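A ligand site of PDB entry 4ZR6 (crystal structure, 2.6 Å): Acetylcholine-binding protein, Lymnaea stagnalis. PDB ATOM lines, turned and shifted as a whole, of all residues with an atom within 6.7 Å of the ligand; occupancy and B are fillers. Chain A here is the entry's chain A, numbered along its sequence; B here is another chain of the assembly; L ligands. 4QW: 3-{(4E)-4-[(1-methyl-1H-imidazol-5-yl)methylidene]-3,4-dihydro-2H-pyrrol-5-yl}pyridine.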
ATOM      1  N   TYR A  97     -34.309 -28.891   5.381  1.00  0.00           N
ATOM      2  CA  TYR A  97     -34.362 -30.117   6.167  1.00  0.00           C
ATOM      3  C   TYR A  97     -35.300 -31.141   5.581  1.00  0.00           C
ATOM      4  O   TYR A  97     -35.096 -32.329   5.802  1.00  0.00           O
ATOM      5  CB  TYR A  97     -34.766 -29.839   7.619  1.00  0.00           C
ATOM      6  CG  TYR A  97     -33.983 -28.742   8.277  1.00  0.00           C
ATOM      7  CD1 TYR A  97     -32.741 -28.351   7.796  1.00  0.00           C
ATOM      8  CD2 TYR A  97     -34.472 -28.090   9.392  1.00  0.00           C
ATOM      9  CE1 TYR A  97     -32.025 -27.340   8.394  1.00  0.00           C
ATOM     10  CE2 TYR A  97     -33.771 -27.069  10.006  1.00  0.00           C
ATOM     11  CZ  TYR A  97     -32.548 -26.694   9.507  1.00  0.00           C
ATOM     12  OH  TYR A  97     -31.831 -25.684  10.104  1.00  0.00           O
ATOM     13  N   GLY A 149     -32.217 -23.715   7.026  1.00  0.00           N
ATOM     14  CA  GLY A 149     -31.331 -23.263   8.092  1.00  0.00           C
ATOM     15  C   GLY A 149     -29.886 -23.602   7.797  1.00  0.00           C
ATOM     16  O   GLY A 149     -29.593 -24.270   6.800  1.00  0.00           O
ATOM     17  N   SER A 150     -28.952 -23.126   8.626  1.00  0.00           N
ATOM     18  CA  SER A 150     -27.566 -23.542   8.486  1.00  0.00           C
ATOM     19  C   SER A 150     -27.427 -24.984   8.918  1.00  0.00           C
ATOM     20  O   SER A 150     -28.071 -25.421   9.867  1.00  0.00           O
ATOM     21  CB  SER A 150     -26.637 -22.680   9.318  1.00  0.00           C
ATOM     22  OG  SER A 150     -25.351 -23.283   9.370  1.00  0.00           O
ATOM     23  N   TRP A 151     -26.575 -25.742   8.266  1.00  0.00           N
ATOM     24  CA  TRP A 151     -26.418 -27.119   8.739  1.00  0.00           C
ATOM     25  C   TRP A 151     -25.385 -27.247   9.858  1.00  0.00           C
ATOM     26  O   TRP A 151     -25.624 -27.978  10.808  1.00  0.00           O
ATOM     27  CB  TRP A 151     -26.076 -28.062   7.579  1.00  0.00           C
ATOM     28  CG  TRP A 151     -26.201 -29.524   7.932  1.00  0.00           C
ATOM     29  CD1 TRP A 151     -25.170 -30.426   8.079  1.00  0.00           C
ATOM     30  CD2 TRP A 151     -27.418 -30.271   8.162  1.00  0.00           C
ATOM     31  NE1 TRP A 151     -25.679 -31.675   8.393  1.00  0.00           N
ATOM     32  CE2 TRP A 151     -27.054 -31.596   8.448  1.00  0.00           C
ATOM     33  CE3 TRP A 151     -28.762 -29.938   8.153  1.00  0.00           C
ATOM     34  CZ2 TRP A 151     -28.004 -32.593   8.725  1.00  0.00           C
ATOM     35  CZ3 TRP A 151     -29.700 -30.917   8.436  1.00  0.00           C
ATOM     36  CH2 TRP A 151     -29.309 -32.225   8.711  1.00  0.00           C
ATOM     37  N   THR A 152     -24.246 -26.567   9.810  1.00  0.00           N
ATOM     38  CA  THR A 152     -23.258 -26.827  10.875  1.00  0.00           C
ATOM     39  C   THR A 152     -22.973 -25.672  11.830  1.00  0.00           C
ATOM     40  O   THR A 152     -22.107 -25.787  12.705  1.00  0.00           O
ATOM     41  CB  THR A 152     -21.899 -27.252  10.309  1.00  0.00           C
ATOM     42  OG1 THR A 152     -21.392 -26.201   9.473  1.00  0.00           O
ATOM     43  CG2 THR A 152     -22.052 -28.537   9.494  1.00  0.00           C
ATOM     44  N   HIS A 153     -23.696 -24.564  11.668  1.00  0.00           N
ATOM     45  CA  HIS A 153     -23.513 -23.398  12.522  1.00  0.00           C
ATOM     46  C   HIS A 153     -24.708 -23.165  13.441  1.00  0.00           C
ATOM     47  O   HIS A 153     -25.852 -23.204  12.989  1.00  0.00           O
ATOM     48  CB  HIS A 153     -23.262 -22.161  11.672  1.00  0.00           C
ATOM     49  CG  HIS A 153     -22.007 -22.229  10.868  1.00  0.00           C
ATOM     50  ND1 HIS A 153     -20.773 -21.915  11.396  1.00  0.00           N
ATOM     51  CD2 HIS A 153     -21.800 -22.515   9.566  1.00  0.00           C
ATOM     52  CE1 HIS A 153     -19.861 -22.028  10.450  1.00  0.00           C
ATOM     53  NE2 HIS A 153     -20.444 -22.392   9.330  1.00  0.00           N
ATOM     54  N   VAL A 191     -34.447 -24.333  17.034  1.00  0.00           N
ATOM     55  CA  VAL A 191     -34.633 -25.719  17.410  1.00  0.00           C
ATOM     56  C   VAL A 191     -33.349 -26.288  18.007  1.00  0.00           C
ATOM     57  O   VAL A 191     -32.253 -26.010  17.520  1.00  0.00           O
ATOM     58  CB  VAL A 191     -35.090 -26.557  16.211  1.00  0.00           C
ATOM     59  CG1 VAL A 191     -35.519 -27.949  16.657  1.00  0.00           C
ATOM     60  CG2 VAL A 191     -36.229 -25.846  15.514  1.00  0.00           C
ATOM     61  N   TYR A 193     -31.723 -29.946  18.831  1.00  0.00           N
ATOM     62  CA  TYR A 193     -31.911 -31.365  18.553  1.00  0.00           C
ATOM     63  C   TYR A 193     -31.344 -32.175  19.705  1.00  0.00           C
ATOM     64  O   TYR A 193     -30.582 -31.656  20.524  1.00  0.00           O
ATOM     65  CB  TYR A 193     -31.267 -31.712  17.209  1.00  0.00           C
ATOM     66  CG  TYR A 193     -31.882 -30.890  16.104  1.00  0.00           C
ATOM     67  CD1 TYR A 193     -31.438 -29.607  15.831  1.00  0.00           C
ATOM     68  CD2 TYR A 193     -32.961 -31.377  15.370  1.00  0.00           C
ATOM     69  CE1 TYR A 193     -32.011 -28.851  14.846  1.00  0.00           C
ATOM     70  CE2 TYR A 193     -33.535 -30.631  14.384  1.00  0.00           C
ATOM     71  CZ  TYR A 193     -33.054 -29.353  14.125  1.00  0.00           C
ATOM     72  OH  TYR A 193     -33.634 -28.576  13.138  1.00  0.00           O
ATOM     73  N   CYS A 195     -29.210 -34.701  19.814  1.00  0.00           N
ATOM     74  CA  CYS A 195     -27.778 -35.024  19.707  1.00  0.00           C
ATOM     75  C   CYS A 195     -26.846 -33.992  20.312  1.00  0.00           C
ATOM     76  O   CYS A 195     -25.817 -34.353  20.874  1.00  0.00           O
ATOM     77  CB  CYS A 195     -27.390 -35.228  18.241  1.00  0.00           C
ATOM     78  SG  CYS A 195     -26.813 -33.760  17.395  1.00  0.00           S
ATOM     79  N   CYS A 196     -27.207 -32.720  20.174  1.00  0.00           N
ATOM     80  CA  CYS A 196     -26.309 -31.605  20.470  1.00  0.00           C
ATOM     81  C   CYS A 196     -27.082 -30.452  21.136  1.00  0.00           C
ATOM     82  O   CYS A 196     -28.248 -30.237  20.825  1.00  0.00           O
ATOM     83  CB  CYS A 196     -25.638 -31.111  19.182  1.00  0.00           C
ATOM     84  SG  CYS A 196     -25.366 -32.371  17.929  1.00  0.00           S
ATOM     85  N   PRO A 197     -26.442 -29.714  22.057  1.00  0.00           N
ATOM     86  CA  PRO A 197     -27.209 -28.800  22.897  1.00  0.00           C
ATOM     87  C   PRO A 197     -27.293 -27.374  22.336  1.00  0.00           C
ATOM     88  O   PRO A 197     -28.050 -26.554  22.844  1.00  0.00           O
ATOM     89  CB  PRO A 197     -26.442 -28.820  24.199  1.00  0.00           C
ATOM     90  CG  PRO A 197     -25.000 -28.942  23.740  1.00  0.00           C
ATOM     91  CD  PRO A 197     -25.008 -29.694  22.414  1.00  0.00           C
ATOM     92  N   GLU A 198     -26.501 -27.100  21.297  1.00  0.00           N
ATOM     93  CA  GLU A 198     -26.598 -25.831  20.586  1.00  0.00           C
ATOM     94  C   GLU A 198     -27.955 -25.699  19.880  1.00  0.00           C
ATOM     95  O   GLU A 198     -28.670 -26.692  19.668  1.00  0.00           O
ATOM     96  CB  GLU A 198     -25.458 -25.703  19.564  1.00  0.00           C
ATOM     97  N   TYR A 200     -30.327 -24.239  16.593  1.00  0.00           N
ATOM     98  CA  TYR A 200     -30.262 -23.950  15.165  1.00  0.00           C
ATOM     99  C   TYR A 200     -31.496 -23.200  14.744  1.00  0.00           C
ATOM    100  O   TYR A 200     -32.620 -23.611  15.044  1.00  0.00           O
ATOM    101  CB  TYR A 200     -30.083 -25.237  14.357  1.00  0.00           C
ATOM    102  CG  TYR A 200     -28.800 -25.918  14.735  1.00  0.00           C
ATOM    103  CD1 TYR A 200     -28.735 -26.723  15.849  1.00  0.00           C
ATOM    104  CD2 TYR A 200     -27.626 -25.680  14.020  1.00  0.00           C
ATOM    105  CE1 TYR A 200     -27.571 -27.309  16.240  1.00  0.00           C
ATOM    106  CE2 TYR A 200     -26.456 -26.266  14.391  1.00  0.00           C
ATOM    107  CZ  TYR A 200     -26.425 -27.096  15.502  1.00  0.00           C
ATOM    108  OH  TYR A 200     -25.254 -27.693  15.895  1.00  0.00           O
ATOM    109  N   GLU A 201     -31.269 -22.078  14.084  1.00  0.00           N
ATOM    110  CA  GLU A 201     -32.345 -21.232  13.598  1.00  0.00           C
ATOM    111  C   GLU A 201     -32.753 -21.684  12.198  1.00  0.00           C
ATOM    112  O   GLU A 201     -31.883 -22.016  11.388  1.00  0.00           O
ATOM    113  CB  GLU A 201     -31.915 -19.758  13.594  1.00  0.00           C
ATOM    114  N   TRP B  61     -30.067 -39.434   8.594  1.00  0.00           N
ATOM    115  CA  TRP B  61     -28.900 -38.701   9.050  1.00  0.00           C
ATOM    116  C   TRP B  61     -27.942 -39.709   9.582  1.00  0.00           C
ATOM    117  O   TRP B  61     -28.326 -40.559  10.375  1.00  0.00           O
ATOM    118  CB  TRP B  61     -29.232 -37.693  10.152  1.00  0.00           C
ATOM    119  CG  TRP B  61     -30.216 -36.661   9.730  1.00  0.00           C
ATOM    120  CD1 TRP B  61     -30.573 -36.343   8.465  1.00  0.00           C
ATOM    121  CD2 TRP B  61     -30.994 -35.820  10.595  1.00  0.00           C
ATOM    122  NE1 TRP B  61     -31.516 -35.344   8.473  1.00  0.00           N
ATOM    123  CE2 TRP B  61     -31.800 -35.008   9.770  1.00  0.00           C
ATOM    124  CE3 TRP B  61     -31.093 -35.666  11.985  1.00  0.00           C
ATOM    125  CZ2 TRP B  61     -32.694 -34.061  10.296  1.00  0.00           C
ATOM    126  CZ3 TRP B  61     -31.984 -34.719  12.502  1.00  0.00           C
ATOM    127  CH2 TRP B  61     -32.764 -33.928  11.654  1.00  0.00           C
ATOM    128  N   SER B  83     -16.279 -25.185  11.856  1.00  0.00           N
ATOM    129  CA  SER B  83     -16.768 -25.998  10.753  1.00  0.00           C
ATOM    130  C   SER B  83     -15.686 -26.110   9.668  1.00  0.00           C
ATOM    131  O   SER B  83     -15.154 -25.098   9.246  1.00  0.00           O
ATOM    132  CB  SER B  83     -18.038 -25.391  10.163  1.00  0.00           C
ATOM    133  OG  SER B  83     -19.073 -25.344  11.124  1.00  0.00           O
ATOM    134  N   PRO B 108     -24.608 -29.692   3.062  1.00  0.00           N
ATOM    135  CA  PRO B 108     -23.223 -29.269   2.818  1.00  0.00           C
ATOM    136  C   PRO B 108     -22.251 -30.256   3.440  1.00  0.00           C
ATOM    137  O   PRO B 108     -22.457 -30.713   4.563  1.00  0.00           O
ATOM    138  CB  PRO B 108     -23.133 -27.883   3.495  1.00  0.00           C
ATOM    139  CG  PRO B 108     -24.554 -27.407   3.580  1.00  0.00           C
ATOM    140  CD  PRO B 108     -25.415 -28.636   3.721  1.00  0.00           C
ATOM    141  N   LEU B 110     -19.744 -30.551   5.372  1.00  0.00           N
ATOM    142  CA  LEU B 110     -18.943 -29.893   6.404  1.00  0.00           C
ATOM    143  C   LEU B 110     -18.946 -30.703   7.674  1.00  0.00           C
ATOM    144  O   LEU B 110     -20.003 -31.214   8.101  1.00  0.00           O
ATOM    145  CB  LEU B 110     -19.464 -28.500   6.725  1.00  0.00           C
ATOM    146  CG  LEU B 110     -19.242 -27.368   5.732  1.00  0.00           C
ATOM    147  CD1 LEU B 110     -20.068 -26.179   6.176  1.00  0.00           C
ATOM    148  CD2 LEU B 110     -17.775 -27.012   5.676  1.00  0.00           C
ATOM    149  N   ALA B 111     -17.758 -30.784   8.275  1.00  0.00           N
ATOM    150  CA  ALA B 111     -17.536 -31.480   9.538  1.00  0.00           C
ATOM    151  C   ALA B 111     -17.323 -30.472  10.652  1.00  0.00           C
ATOM    152  O   ALA B 111     -16.713 -29.428  10.442  1.00  0.00           O
ATOM    153  CB  ALA B 111     -16.327 -32.393   9.430  1.00  0.00           C
ATOM    154  N   ARG B 112     -17.831 -30.785  11.839  1.00  0.00           N
ATOM    155  CA  ARG B 112     -17.587 -29.969  13.021  1.00  0.00           C
ATOM    156  C   ARG B 112     -16.339 -30.474  13.746  1.00  0.00           C
ATOM    157  O   ARG B 112     -16.213 -31.673  13.969  1.00  0.00           O
ATOM    158  CB  ARG B 112     -18.785 -30.022  13.970  1.00  0.00           C
ATOM    159  CG  ARG B 112     -18.824 -28.913  14.994  1.00  0.00           C
ATOM    160  CD  ARG B 112     -19.250 -27.601  14.375  1.00  0.00           C
ATOM    161  NE  ARG B 112     -19.703 -26.662  15.397  1.00  0.00           N
ATOM    162  CZ  ARG B 112     -19.587 -25.343  15.302  1.00  0.00           C
ATOM    163  NH1 ARG B 112     -19.039 -24.792  14.226  1.00  0.00           N
ATOM    164  NH2 ARG B 112     -20.028 -24.586  16.300  1.00  0.00           N
ATOM    165  N   LEU B 120     -17.036 -34.434  14.339  1.00  0.00           N
ATOM    166  CA  LEU B 120     -18.401 -34.908  14.097  1.00  0.00           C
ATOM    167  C   LEU B 120     -18.866 -34.542  12.677  1.00  0.00           C
ATOM    168  O   LEU B 120     -18.923 -33.360  12.319  1.00  0.00           O
ATOM    169  CB  LEU B 120     -19.393 -34.357  15.127  1.00  0.00           C
ATOM    170  CG  LEU B 120     -20.846 -34.454  14.642  1.00  0.00           C
ATOM    171  CD1 LEU B 120     -21.346 -35.909  14.524  1.00  0.00           C
ATOM    172  CD2 LEU B 120     -21.810 -33.649  15.500  1.00  0.00           C
ATOM    173  N   TYR B 121     -19.197 -35.554  11.882  1.00  0.00           N
ATOM    174  CA  TYR B 121     -19.743 -35.387  10.540  1.00  0.00           C
ATOM    175  C   TYR B 121     -21.125 -36.067  10.487  1.00  0.00           C
ATOM    176  O   TYR B 121     -21.251 -37.251  10.787  1.00  0.00           O
ATOM    177  CB  TYR B 121     -18.760 -35.956   9.496  1.00  0.00           C
ATOM    178  CG  TYR B 121     -19.210 -35.832   8.050  1.00  0.00           C
ATOM    179  CD1 TYR B 121     -19.724 -34.632   7.565  1.00  0.00           C
ATOM    180  CD2 TYR B 121     -19.101 -36.912   7.171  1.00  0.00           C
ATOM    181  CE1 TYR B 121     -20.139 -34.524   6.249  1.00  0.00           C
ATOM    182  CE2 TYR B 121     -19.502 -36.796   5.851  1.00  0.00           C
ATOM    183  CZ  TYR B 121     -20.030 -35.597   5.402  1.00  0.00           C
ATOM    184  OH  TYR B 121     -20.461 -35.447   4.093  1.00  0.00           O
ATOM    185  N   MET B 122     -22.159 -35.309  10.141  1.00  0.00           N
ATOM    186  CA  MET B 122     -23.518 -35.870  10.079  1.00  0.00           C
ATOM    187  C   MET B 122     -24.314 -35.459   8.847  1.00  0.00           C
ATOM    188  O   MET B 122     -25.157 -34.581   8.941  1.00  0.00           O
ATOM    189  CB  MET B 122     -24.337 -35.470  11.306  1.00  0.00           C
ATOM    190  CG  MET B 122     -25.627 -36.268  11.422  1.00  0.00           C
ATOM    191  SD  MET B 122     -26.584 -35.943  12.904  1.00  0.00           S
ATOM    192  CE  MET B 122     -27.161 -34.298  12.519  1.00  0.00           C
ATOM    193  N   PRO B 123     -24.055 -36.079   7.701  1.00  0.00           N
ATOM    194  CA  PRO B 123     -24.787 -35.580   6.539  1.00  0.00           C
ATOM    195  C   PRO B 123     -26.184 -36.187   6.472  1.00  0.00           C
ATOM    196  O   PRO B 123     -26.434 -37.214   7.117  1.00  0.00           O
ATOM    197  CB  PRO B 123     -23.924 -36.030   5.347  1.00  0.00           C
ATOM    198  CG  PRO B 123     -23.140 -37.227   5.860  1.00  0.00           C
ATOM    199  CD  PRO B 123     -23.014 -37.060   7.346  1.00  0.00           C
HETATM  200  C10 4QW L   1     -27.209 -30.548  15.613  1.00  0.00           C
HETATM  201  C13 4QW L   1     -24.501 -31.046  13.017  1.00  0.00           C
HETATM  202  C15 4QW L   1     -22.165 -30.615  12.798  1.00  0.00           C
HETATM  203  C01 4QW L   1     -30.716 -30.938  11.976  1.00  0.00           C
HETATM  204  N02 4QW L   1     -29.941 -29.752  11.876  1.00  0.00           N
HETATM  205  C03 4QW L   1     -30.409 -28.503  11.698  1.00  0.00           C
HETATM  206  N04 4QW L   1     -29.390 -27.636  11.645  1.00  0.00           N
HETATM  207  C05 4QW L   1     -28.266 -28.328  11.803  1.00  0.00           C
HETATM  208  C06 4QW L   1     -28.606 -29.674  11.941  1.00  0.00           C
HETATM  209  C07 4QW L   1     -27.627 -30.825  12.122  1.00  0.00           C
HETATM  210  C08 4QW L   1     -27.158 -31.195  13.351  1.00  0.00           C
HETATM  211  C09 4QW L   1     -27.983 -31.339  14.565  1.00  0.00           C
HETATM  212  N11 4QW L   1     -25.803 -30.569  15.209  1.00  0.00           N
HETATM  213  C12 4QW L   1     -25.760 -31.030  13.839  1.00  0.00           C
HETATM  214  C14 4QW L   1     -23.316 -30.597  13.564  1.00  0.00           C
HETATM  215  C16 4QW L   1     -22.246 -31.087  11.498  1.00  0.00           C
HETATM  216  N17 4QW L   1     -23.394 -31.523  10.975  1.00  0.00           N
HETATM  217  C18 4QW L   1     -24.524 -31.515  11.707  1.00  0.00           C
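N17 of the ligand sits at hydrogen-bond distance from NE1 of Trp 151, at 3.5 Å. A nitrogen (N04) of the ligand sits at hydrogen-bond distance from the side-chain hydroxyl (OH) of Tyr 97 (3.5 Å). N11 of the ligand sits at hydrogen-bond distance from OH of Tyr 200 (3.0 Å).
The side-chain sulfur (SG) of Cys 195 forms a disulfide with the side-chain sulfur (SG) of Cys 196, 2.1 Å away. The backbone carbonyl oxygen (O) of Val 191 sits at hydrogen-bond distance from the backbone NH (N) of Tyr 200. The backbone carbonyl oxygen of Met 122 of chain B sits at hydrogen-bond distance from the indole nitrogen of Trp 151, at 3.0 Å. The side-chain hydroxyl (OG) of Ser 150 sits at hydrogen-bond distance from the backbone NH (N) of His 153 (3.1 Å). The guanidinium group of Arg 112 of chain B sits at hydrogen-bond distance from the side-chain hydroxyl of Ser 83 of chain B (3.2 Å). The side-chain hydroxyl (OG1) of Thr 152 lies within hydrogen-bond range of the side-chain hydroxyl (OG) of Ser 83 of chain B (3.0 Å). OG of Ser 150 sits at hydrogen-bond distance from N of Thr 152, 3.5 Å away. The backbone NH (N) of Arg 112 of chain B lies within hydrogen-bond range of the backbone carbonyl oxygen (O) of Leu 120 of chain B (2.8 Å).
The backbone carbonyl oxygen (O) of Ser 150 sits close to a nitrogen (N04) of the ligand, 3.1 Å away. SG of Cys 196 lies close to N11 of the ligand, at 3.3 Å. Merely in contact with the ligand: Met 122 of chain B (3.2 Å), Thr 152 (3.2 Å), Tyr 193 (3.5 Å), Arg 112 of chain B (3.6 Å), Trp 61 of chain B (3.6 Å), Cys 195 (3.7 Å) and Leu 120 of chain B (3.9 Å). The nearest printed residue that does not touch the ligand is Leu 110 of chain B (4.1 Å).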
